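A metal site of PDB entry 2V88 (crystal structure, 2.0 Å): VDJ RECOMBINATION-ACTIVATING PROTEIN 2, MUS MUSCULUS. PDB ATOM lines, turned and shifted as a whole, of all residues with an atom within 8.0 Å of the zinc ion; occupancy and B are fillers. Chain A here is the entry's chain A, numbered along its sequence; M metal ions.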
ATOM      1  N   TYR A  10     -12.378  19.685 -24.158  1.00  0.00           N
ATOM      2  CA  TYR A  10     -11.696  18.708 -23.334  1.00  0.00           C
ATOM      3  C   TYR A  10     -10.308  18.331 -23.867  1.00  0.00           C
ATOM      4  O   TYR A  10      -9.467  17.836 -23.113  1.00  0.00           O
ATOM      5  CB  TYR A  10     -12.538  17.424 -23.256  1.00  0.00           C
ATOM      6  CG  TYR A  10     -13.761  17.497 -22.386  1.00  0.00           C
ATOM      7  CD1 TYR A  10     -15.008  17.833 -22.918  1.00  0.00           C
ATOM      8  CD2 TYR A  10     -13.687  17.207 -21.023  1.00  0.00           C
ATOM      9  CE1 TYR A  10     -16.149  17.859 -22.110  1.00  0.00           C
ATOM     10  CE2 TYR A  10     -14.818  17.232 -20.219  1.00  0.00           C
ATOM     11  CZ  TYR A  10     -16.038  17.554 -20.764  1.00  0.00           C
ATOM     12  OH  TYR A  10     -17.159  17.544 -19.960  1.00  0.00           O
ATOM     13  N   TRP A  11     -10.069  18.571 -25.148  1.00  0.00           N
ATOM     14  CA  TRP A  11      -8.802  18.178 -25.742  1.00  0.00           C
ATOM     15  C   TRP A  11      -7.756  19.261 -25.979  1.00  0.00           C
ATOM     16  O   TRP A  11      -6.980  19.200 -26.912  1.00  0.00           O
ATOM     17  CB  TRP A  11      -9.078  17.388 -27.024  1.00  0.00           C
ATOM     18  CG  TRP A  11     -10.068  16.293 -26.758  1.00  0.00           C
ATOM     19  CD1 TRP A  11     -11.353  16.225 -27.214  1.00  0.00           C
ATOM     20  CD2 TRP A  11      -9.876  15.158 -25.914  1.00  0.00           C
ATOM     21  NE1 TRP A  11     -11.971  15.109 -26.693  1.00  0.00           N
ATOM     22  CE2 TRP A  11     -11.094  14.438 -25.897  1.00  0.00           C
ATOM     23  CE3 TRP A  11      -8.800  14.666 -25.163  1.00  0.00           C
ATOM     24  CZ2 TRP A  11     -11.255  13.265 -25.153  1.00  0.00           C
ATOM     25  CZ3 TRP A  11      -8.964  13.501 -24.425  1.00  0.00           C
ATOM     26  CH2 TRP A  11     -10.181  12.812 -24.434  1.00  0.00           C
ATOM     27  N   ILE A  12      -7.740  20.258 -25.104  1.00  0.00           N
ATOM     28  CA  ILE A  12      -6.770  21.336 -25.181  1.00  0.00           C
ATOM     29  C   ILE A  12      -5.460  20.866 -24.544  1.00  0.00           C
ATOM     30  O   ILE A  12      -5.384  19.783 -23.962  1.00  0.00           O
ATOM     31  CB  ILE A  12      -7.220  22.559 -24.369  1.00  0.00           C
ATOM     32  CG1 ILE A  12      -7.549  22.103 -22.931  1.00  0.00           C
ATOM     33  CG2 ILE A  12      -8.412  23.216 -25.009  1.00  0.00           C
ATOM     34  CD1 ILE A  12      -7.878  23.236 -21.979  1.00  0.00           C
ATOM     35  N   THR A  13      -4.430  21.685 -24.681  1.00  0.00           N
ATOM     36  CA  THR A  13      -3.159  21.401 -24.038  1.00  0.00           C
ATOM     37  C   THR A  13      -3.310  22.393 -22.883  1.00  0.00           C
ATOM     38  O   THR A  13      -3.109  23.587 -23.050  1.00  0.00           O
ATOM     39  CB  THR A  13      -1.976  21.776 -24.963  1.00  0.00           C
ATOM     40  OG1 THR A  13      -1.969  20.896 -26.102  1.00  0.00           O
ATOM     41  CG2 THR A  13      -0.654  21.644 -24.223  1.00  0.00           C
ATOM     42  N   CYS A  14      -3.705  21.880 -21.716  1.00  0.00           N
ATOM     43  CA  CYS A  14      -3.985  22.721 -20.557  1.00  0.00           C
ATOM     44  C   CYS A  14      -2.839  23.448 -19.870  1.00  0.00           C
ATOM     45  O   CYS A  14      -3.063  24.446 -19.190  1.00  0.00           O
ATOM     46  CB  CYS A  14      -4.772  21.931 -19.501  1.00  0.00           C
ATOM     47  SG  CYS A  14      -3.786  20.910 -18.375  1.00  0.00           S
ATOM     48  N   CYS A  15      -1.627  22.943 -20.010  1.00  0.00           N
ATOM     49  CA  CYS A  15      -0.464  23.562 -19.388  1.00  0.00           C
ATOM     50  C   CYS A  15       0.813  23.048 -20.062  1.00  0.00           C
ATOM     51  O   CYS A  15       0.770  22.163 -20.897  1.00  0.00           O
ATOM     52  CB  CYS A  15      -0.442  23.247 -17.885  1.00  0.00           C
ATOM     53  SG  CYS A  15      -0.254  21.501 -17.493  1.00  0.00           S
ATOM     54  N   PRO A  16       1.972  23.629 -19.712  1.00  0.00           N
ATOM     55  CA  PRO A  16       3.241  23.214 -20.301  1.00  0.00           C
ATOM     56  C   PRO A  16       3.568  21.714 -20.237  1.00  0.00           C
ATOM     57  O   PRO A  16       4.257  21.197 -21.110  1.00  0.00           O
ATOM     58  CB  PRO A  16       4.258  24.054 -19.535  1.00  0.00           C
ATOM     59  CG  PRO A  16       3.508  25.326 -19.309  1.00  0.00           C
ATOM     60  CD  PRO A  16       2.154  24.826 -18.858  1.00  0.00           C
ATOM     61  N   THR A  17       3.072  21.027 -19.210  1.00  0.00           N
ATOM     62  CA  THR A  17       3.350  19.606 -19.055  1.00  0.00           C
ATOM     63  C   THR A  17       2.142  18.695 -19.278  1.00  0.00           C
ATOM     64  O   THR A  17       2.203  17.518 -18.970  1.00  0.00           O
ATOM     65  CB  THR A  17       3.924  19.311 -17.657  1.00  0.00           C
ATOM     66  OG1 THR A  17       3.029  19.789 -16.651  1.00  0.00           O
ATOM     67  CG2 THR A  17       5.271  19.993 -17.486  1.00  0.00           C
ATOM     68  N   CYS A  18       1.060  19.246 -19.829  1.00  0.00           N
ATOM     69  CA  CYS A  18      -0.171  18.495 -20.086  1.00  0.00           C
ATOM     70  C   CYS A  18       0.050  17.123 -20.715  1.00  0.00           C
ATOM     71  O   CYS A  18       0.658  17.011 -21.770  1.00  0.00           O
ATOM     72  CB  CYS A  18      -1.101  19.329 -20.988  1.00  0.00           C
ATOM     73  SG  CYS A  18      -2.660  18.513 -21.441  1.00  0.00           S
ATOM     74  N   ASP A  19      -0.492  16.104 -20.060  1.00  0.00           N
ATOM     75  CA  ASP A  19      -0.377  14.704 -20.497  1.00  0.00           C
ATOM     76  C   ASP A  19      -1.651  14.179 -21.155  1.00  0.00           C
ATOM     77  O   ASP A  19      -1.701  13.030 -21.604  1.00  0.00           O
ATOM     78  CB  ASP A  19      -0.069  13.814 -19.289  1.00  0.00           C
ATOM     79  CG  ASP A  19       1.400  13.838 -18.913  1.00  0.00           C
ATOM     80  OD1 ASP A  19       1.699  13.631 -17.715  1.00  0.00           O
ATOM     81  OD2 ASP A  19       2.245  14.027 -19.814  1.00  0.00           O
ATOM     82  N   VAL A  20      -2.691  15.001 -21.209  1.00  0.00           N
ATOM     83  CA  VAL A  20      -3.934  14.583 -21.821  1.00  0.00           C
ATOM     84  C   VAL A  20      -3.913  14.811 -23.322  1.00  0.00           C
ATOM     85  O   VAL A  20      -3.686  15.917 -23.770  1.00  0.00           O
ATOM     86  CB  VAL A  20      -5.138  15.328 -21.212  1.00  0.00           C
ATOM     87  CG1 VAL A  20      -6.406  14.975 -21.968  1.00  0.00           C
ATOM     88  CG2 VAL A  20      -5.268  14.958 -19.738  1.00  0.00           C
ATOM     89  N   ASP A  21      -4.120  13.741 -24.081  1.00  0.00           N
ATOM     90  CA  ASP A  21      -4.112  13.823 -25.532  1.00  0.00           C
ATOM     91  C   ASP A  21      -5.294  13.033 -26.065  1.00  0.00           C
ATOM     92  O   ASP A  21      -5.598  11.940 -25.569  1.00  0.00           O
ATOM     93  CB  ASP A  21      -2.774  13.249 -26.052  1.00  0.00           C
ATOM     94  CG  ASP A  21      -2.619  13.379 -27.565  1.00  0.00           C
ATOM     95  OD1 ASP A  21      -1.473  13.532 -28.017  1.00  0.00           O
ATOM     96  OD2 ASP A  21      -3.632  13.310 -28.283  1.00  0.00           O
ATOM     97  N   PRO A  36     -11.836  13.447 -20.083  1.00  0.00           N
ATOM     98  CA  PRO A  36     -10.954  13.784 -18.974  1.00  0.00           C
ATOM     99  C   PRO A  36     -11.639  14.732 -17.992  1.00  0.00           C
ATOM    100  O   PRO A  36     -12.359  15.636 -18.403  1.00  0.00           O
ATOM    101  CB  PRO A  36      -9.759  14.420 -19.659  1.00  0.00           C
ATOM    102  CG  PRO A  36     -10.385  15.122 -20.822  1.00  0.00           C
ATOM    103  CD  PRO A  36     -11.405  14.107 -21.324  1.00  0.00           C
ATOM    104  N   ALA A  37     -11.428  14.512 -16.691  1.00  0.00           N
ATOM    105  CA  ALA A  37     -12.019  15.375 -15.687  1.00  0.00           C
ATOM    106  C   ALA A  37     -11.292  16.704 -15.729  1.00  0.00           C
ATOM    107  O   ALA A  37     -10.075  16.753 -15.869  1.00  0.00           O
ATOM    108  CB  ALA A  37     -11.889  14.745 -14.286  1.00  0.00           C
ATOM    109  N   MET A  38     -12.041  17.800 -15.601  1.00  0.00           N
ATOM    110  CA  MET A  38     -11.440  19.115 -15.662  1.00  0.00           C
ATOM    111  C   MET A  38     -11.883  20.037 -14.534  1.00  0.00           C
ATOM    112  O   MET A  38     -12.917  19.827 -13.912  1.00  0.00           O
ATOM    113  CB  MET A  38     -11.752  19.765 -17.034  1.00  0.00           C
ATOM    114  CG  MET A  38     -11.208  18.973 -18.233  1.00  0.00           C
ATOM    115  SD  MET A  38     -11.283  19.894 -19.799  1.00  0.00           S
ATOM    116  CE  MET A  38      -9.758  20.845 -19.700  1.00  0.00           C
ATOM    117  N   TRP A  48      -9.536  26.538 -18.219  1.00  0.00           N
ATOM    118  CA  TRP A  48      -9.758  25.169 -17.780  1.00  0.00           C
ATOM    119  C   TRP A  48      -8.491  24.313 -17.913  1.00  0.00           C
ATOM    120  O   TRP A  48      -7.740  24.454 -18.860  1.00  0.00           O
ATOM    121  CB  TRP A  48     -10.871  24.531 -18.600  1.00  0.00           C
ATOM    122  CG  TRP A  48     -12.241  25.059 -18.317  1.00  0.00           C
ATOM    123  CD1 TRP A  48     -12.863  26.114 -18.943  1.00  0.00           C
ATOM    124  CD2 TRP A  48     -13.178  24.542 -17.370  1.00  0.00           C
ATOM    125  NE1 TRP A  48     -14.134  26.274 -18.435  1.00  0.00           N
ATOM    126  CE2 TRP A  48     -14.351  25.323 -17.459  1.00  0.00           C
ATOM    127  CE3 TRP A  48     -13.134  23.492 -16.442  1.00  0.00           C
ATOM    128  CZ2 TRP A  48     -15.468  25.086 -16.668  1.00  0.00           C
ATOM    129  CZ3 TRP A  48     -14.251  23.254 -15.650  1.00  0.00           C
ATOM    130  CH2 TRP A  48     -15.404  24.045 -15.770  1.00  0.00           C
ATOM    131  N   VAL A  49      -8.281  23.429 -16.949  1.00  0.00           N
ATOM    132  CA  VAL A  49      -7.138  22.519 -16.985  1.00  0.00           C
ATOM    133  C   VAL A  49      -7.608  21.119 -16.626  1.00  0.00           C
ATOM    134  O   VAL A  49      -8.654  20.953 -16.008  1.00  0.00           O
ATOM    135  CB  VAL A  49      -6.021  22.941 -15.992  1.00  0.00           C
ATOM    136  CG1 VAL A  49      -5.440  24.289 -16.394  1.00  0.00           C
ATOM    137  CG2 VAL A  49      -6.553  22.985 -14.561  1.00  0.00           C
ATOM    138  N   HIS A  50      -6.827  20.126 -17.024  1.00  0.00           N
ATOM    139  CA  HIS A  50      -7.181  18.741 -16.725  1.00  0.00           C
ATOM    140  C   HIS A  50      -6.783  18.478 -15.282  1.00  0.00           C
ATOM    141  O   HIS A  50      -5.661  18.773 -14.888  1.00  0.00           O
ATOM    142  CB  HIS A  50      -6.445  17.780 -17.660  1.00  0.00           C
ATOM    143  CG  HIS A  50      -6.744  18.009 -19.100  1.00  0.00           C
ATOM    144  ND1 HIS A  50      -5.802  18.443 -20.006  1.00  0.00           N
ATOM    145  CD2 HIS A  50      -7.895  17.867 -19.810  1.00  0.00           C
ATOM    146  CE1 HIS A  50      -6.348  18.554 -21.199  1.00  0.00           C
ATOM    147  NE2 HIS A  50      -7.626  18.213 -21.098  1.00  0.00           N
ATOM    148  N   ALA A  51      -7.697  17.940 -14.492  1.00  0.00           N
ATOM    149  CA  ALA A  51      -7.398  17.659 -13.104  1.00  0.00           C
ATOM    150  C   ALA A  51      -6.182  16.750 -12.962  1.00  0.00           C
ATOM    151  O   ALA A  51      -5.365  16.946 -12.065  1.00  0.00           O
ATOM    152  CB  ALA A  51      -8.604  17.031 -12.421  1.00  0.00           C
ATOM    153  N   GLN A  52      -6.059  15.754 -13.838  1.00  0.00           N
ATOM    154  CA  GLN A  52      -4.928  14.828 -13.771  1.00  0.00           C
ATOM    155  C   GLN A  52      -3.593  15.532 -13.976  1.00  0.00           C
ATOM    156  O   GLN A  52      -2.605  15.184 -13.341  1.00  0.00           O
ATOM    157  CB  GLN A  52      -5.072  13.702 -14.800  1.00  0.00           C
ATOM    158  CG  GLN A  52      -4.045  12.592 -14.613  1.00  0.00           C
ATOM    159  CD  GLN A  52      -4.214  11.411 -15.569  1.00  0.00           C
ATOM    160  OE1 GLN A  52      -5.242  11.264 -16.214  1.00  0.00           O
ATOM    161  NE2 GLN A  52      -3.202  10.567 -15.637  1.00  0.00           N
ATOM    162  N   CYS A  53      -3.575  16.519 -14.860  1.00  0.00           N
ATOM    163  CA  CYS A  53      -2.363  17.259 -15.157  1.00  0.00           C
ATOM    164  C   CYS A  53      -1.925  18.129 -13.984  1.00  0.00           C
ATOM    165  O   CYS A  53      -0.804  18.620 -13.943  1.00  0.00           O
ATOM    166  CB  CYS A  53      -2.580  18.120 -16.404  1.00  0.00           C
ATOM    167  SG  CYS A  53      -3.008  17.171 -17.874  1.00  0.00           S
ATOM    168  N   MET A  54      -2.830  18.314 -13.023  1.00  0.00           N
ATOM    169  CA  MET A  54      -2.522  19.133 -11.850  1.00  0.00           C
ATOM    170  C   MET A  54      -2.109  18.215 -10.703  1.00  0.00           C
ATOM    171  O   MET A  54      -1.821  18.679  -9.601  1.00  0.00           O
ATOM    172  CB  MET A  54      -3.744  19.948 -11.448  1.00  0.00           C
ATOM    173  CG  MET A  54      -4.237  20.920 -12.526  1.00  0.00           C
ATOM    174  SD  MET A  54      -3.013  22.201 -12.911  1.00  0.00           S
ATOM    175  CE  MET A  54      -2.419  21.657 -14.501  1.00  0.00           C
HETATM  176 ZN    ZN M   1      -3.787  18.780 -19.377  1.00  0.00          ZN
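The zinc ion is bound by ND1 of His 50 (2.1 Å), SG of Cys 53 (2.3 Å), SG of Cys 14 (2.4 Å) and SG of Cys 18 (2.4 Å).
The zinc ion has four donor atoms within binding distance.
Of the 22 residues printed, 4 come within 4 Å of the zinc ion.
The backbone carbonyl oxygen (O) of Tyr 10 lies within hydrogen-bond range of a ring nitrogen (NE2) of His 50, at 2.8 Å.
SG of Cys 15 sits at hydrogen-bond distance from N of Cys 18.
The backbone NH (N) of Asp 19 lies close to the side-chain sulfur (SG) of Cys 53 (3.5 Å).
N of Val 20 sits close to SG of Cys 18, 3.5 Å away.
SG of Cys 14 sits close to SG of Cys 15 (3.7 Å).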
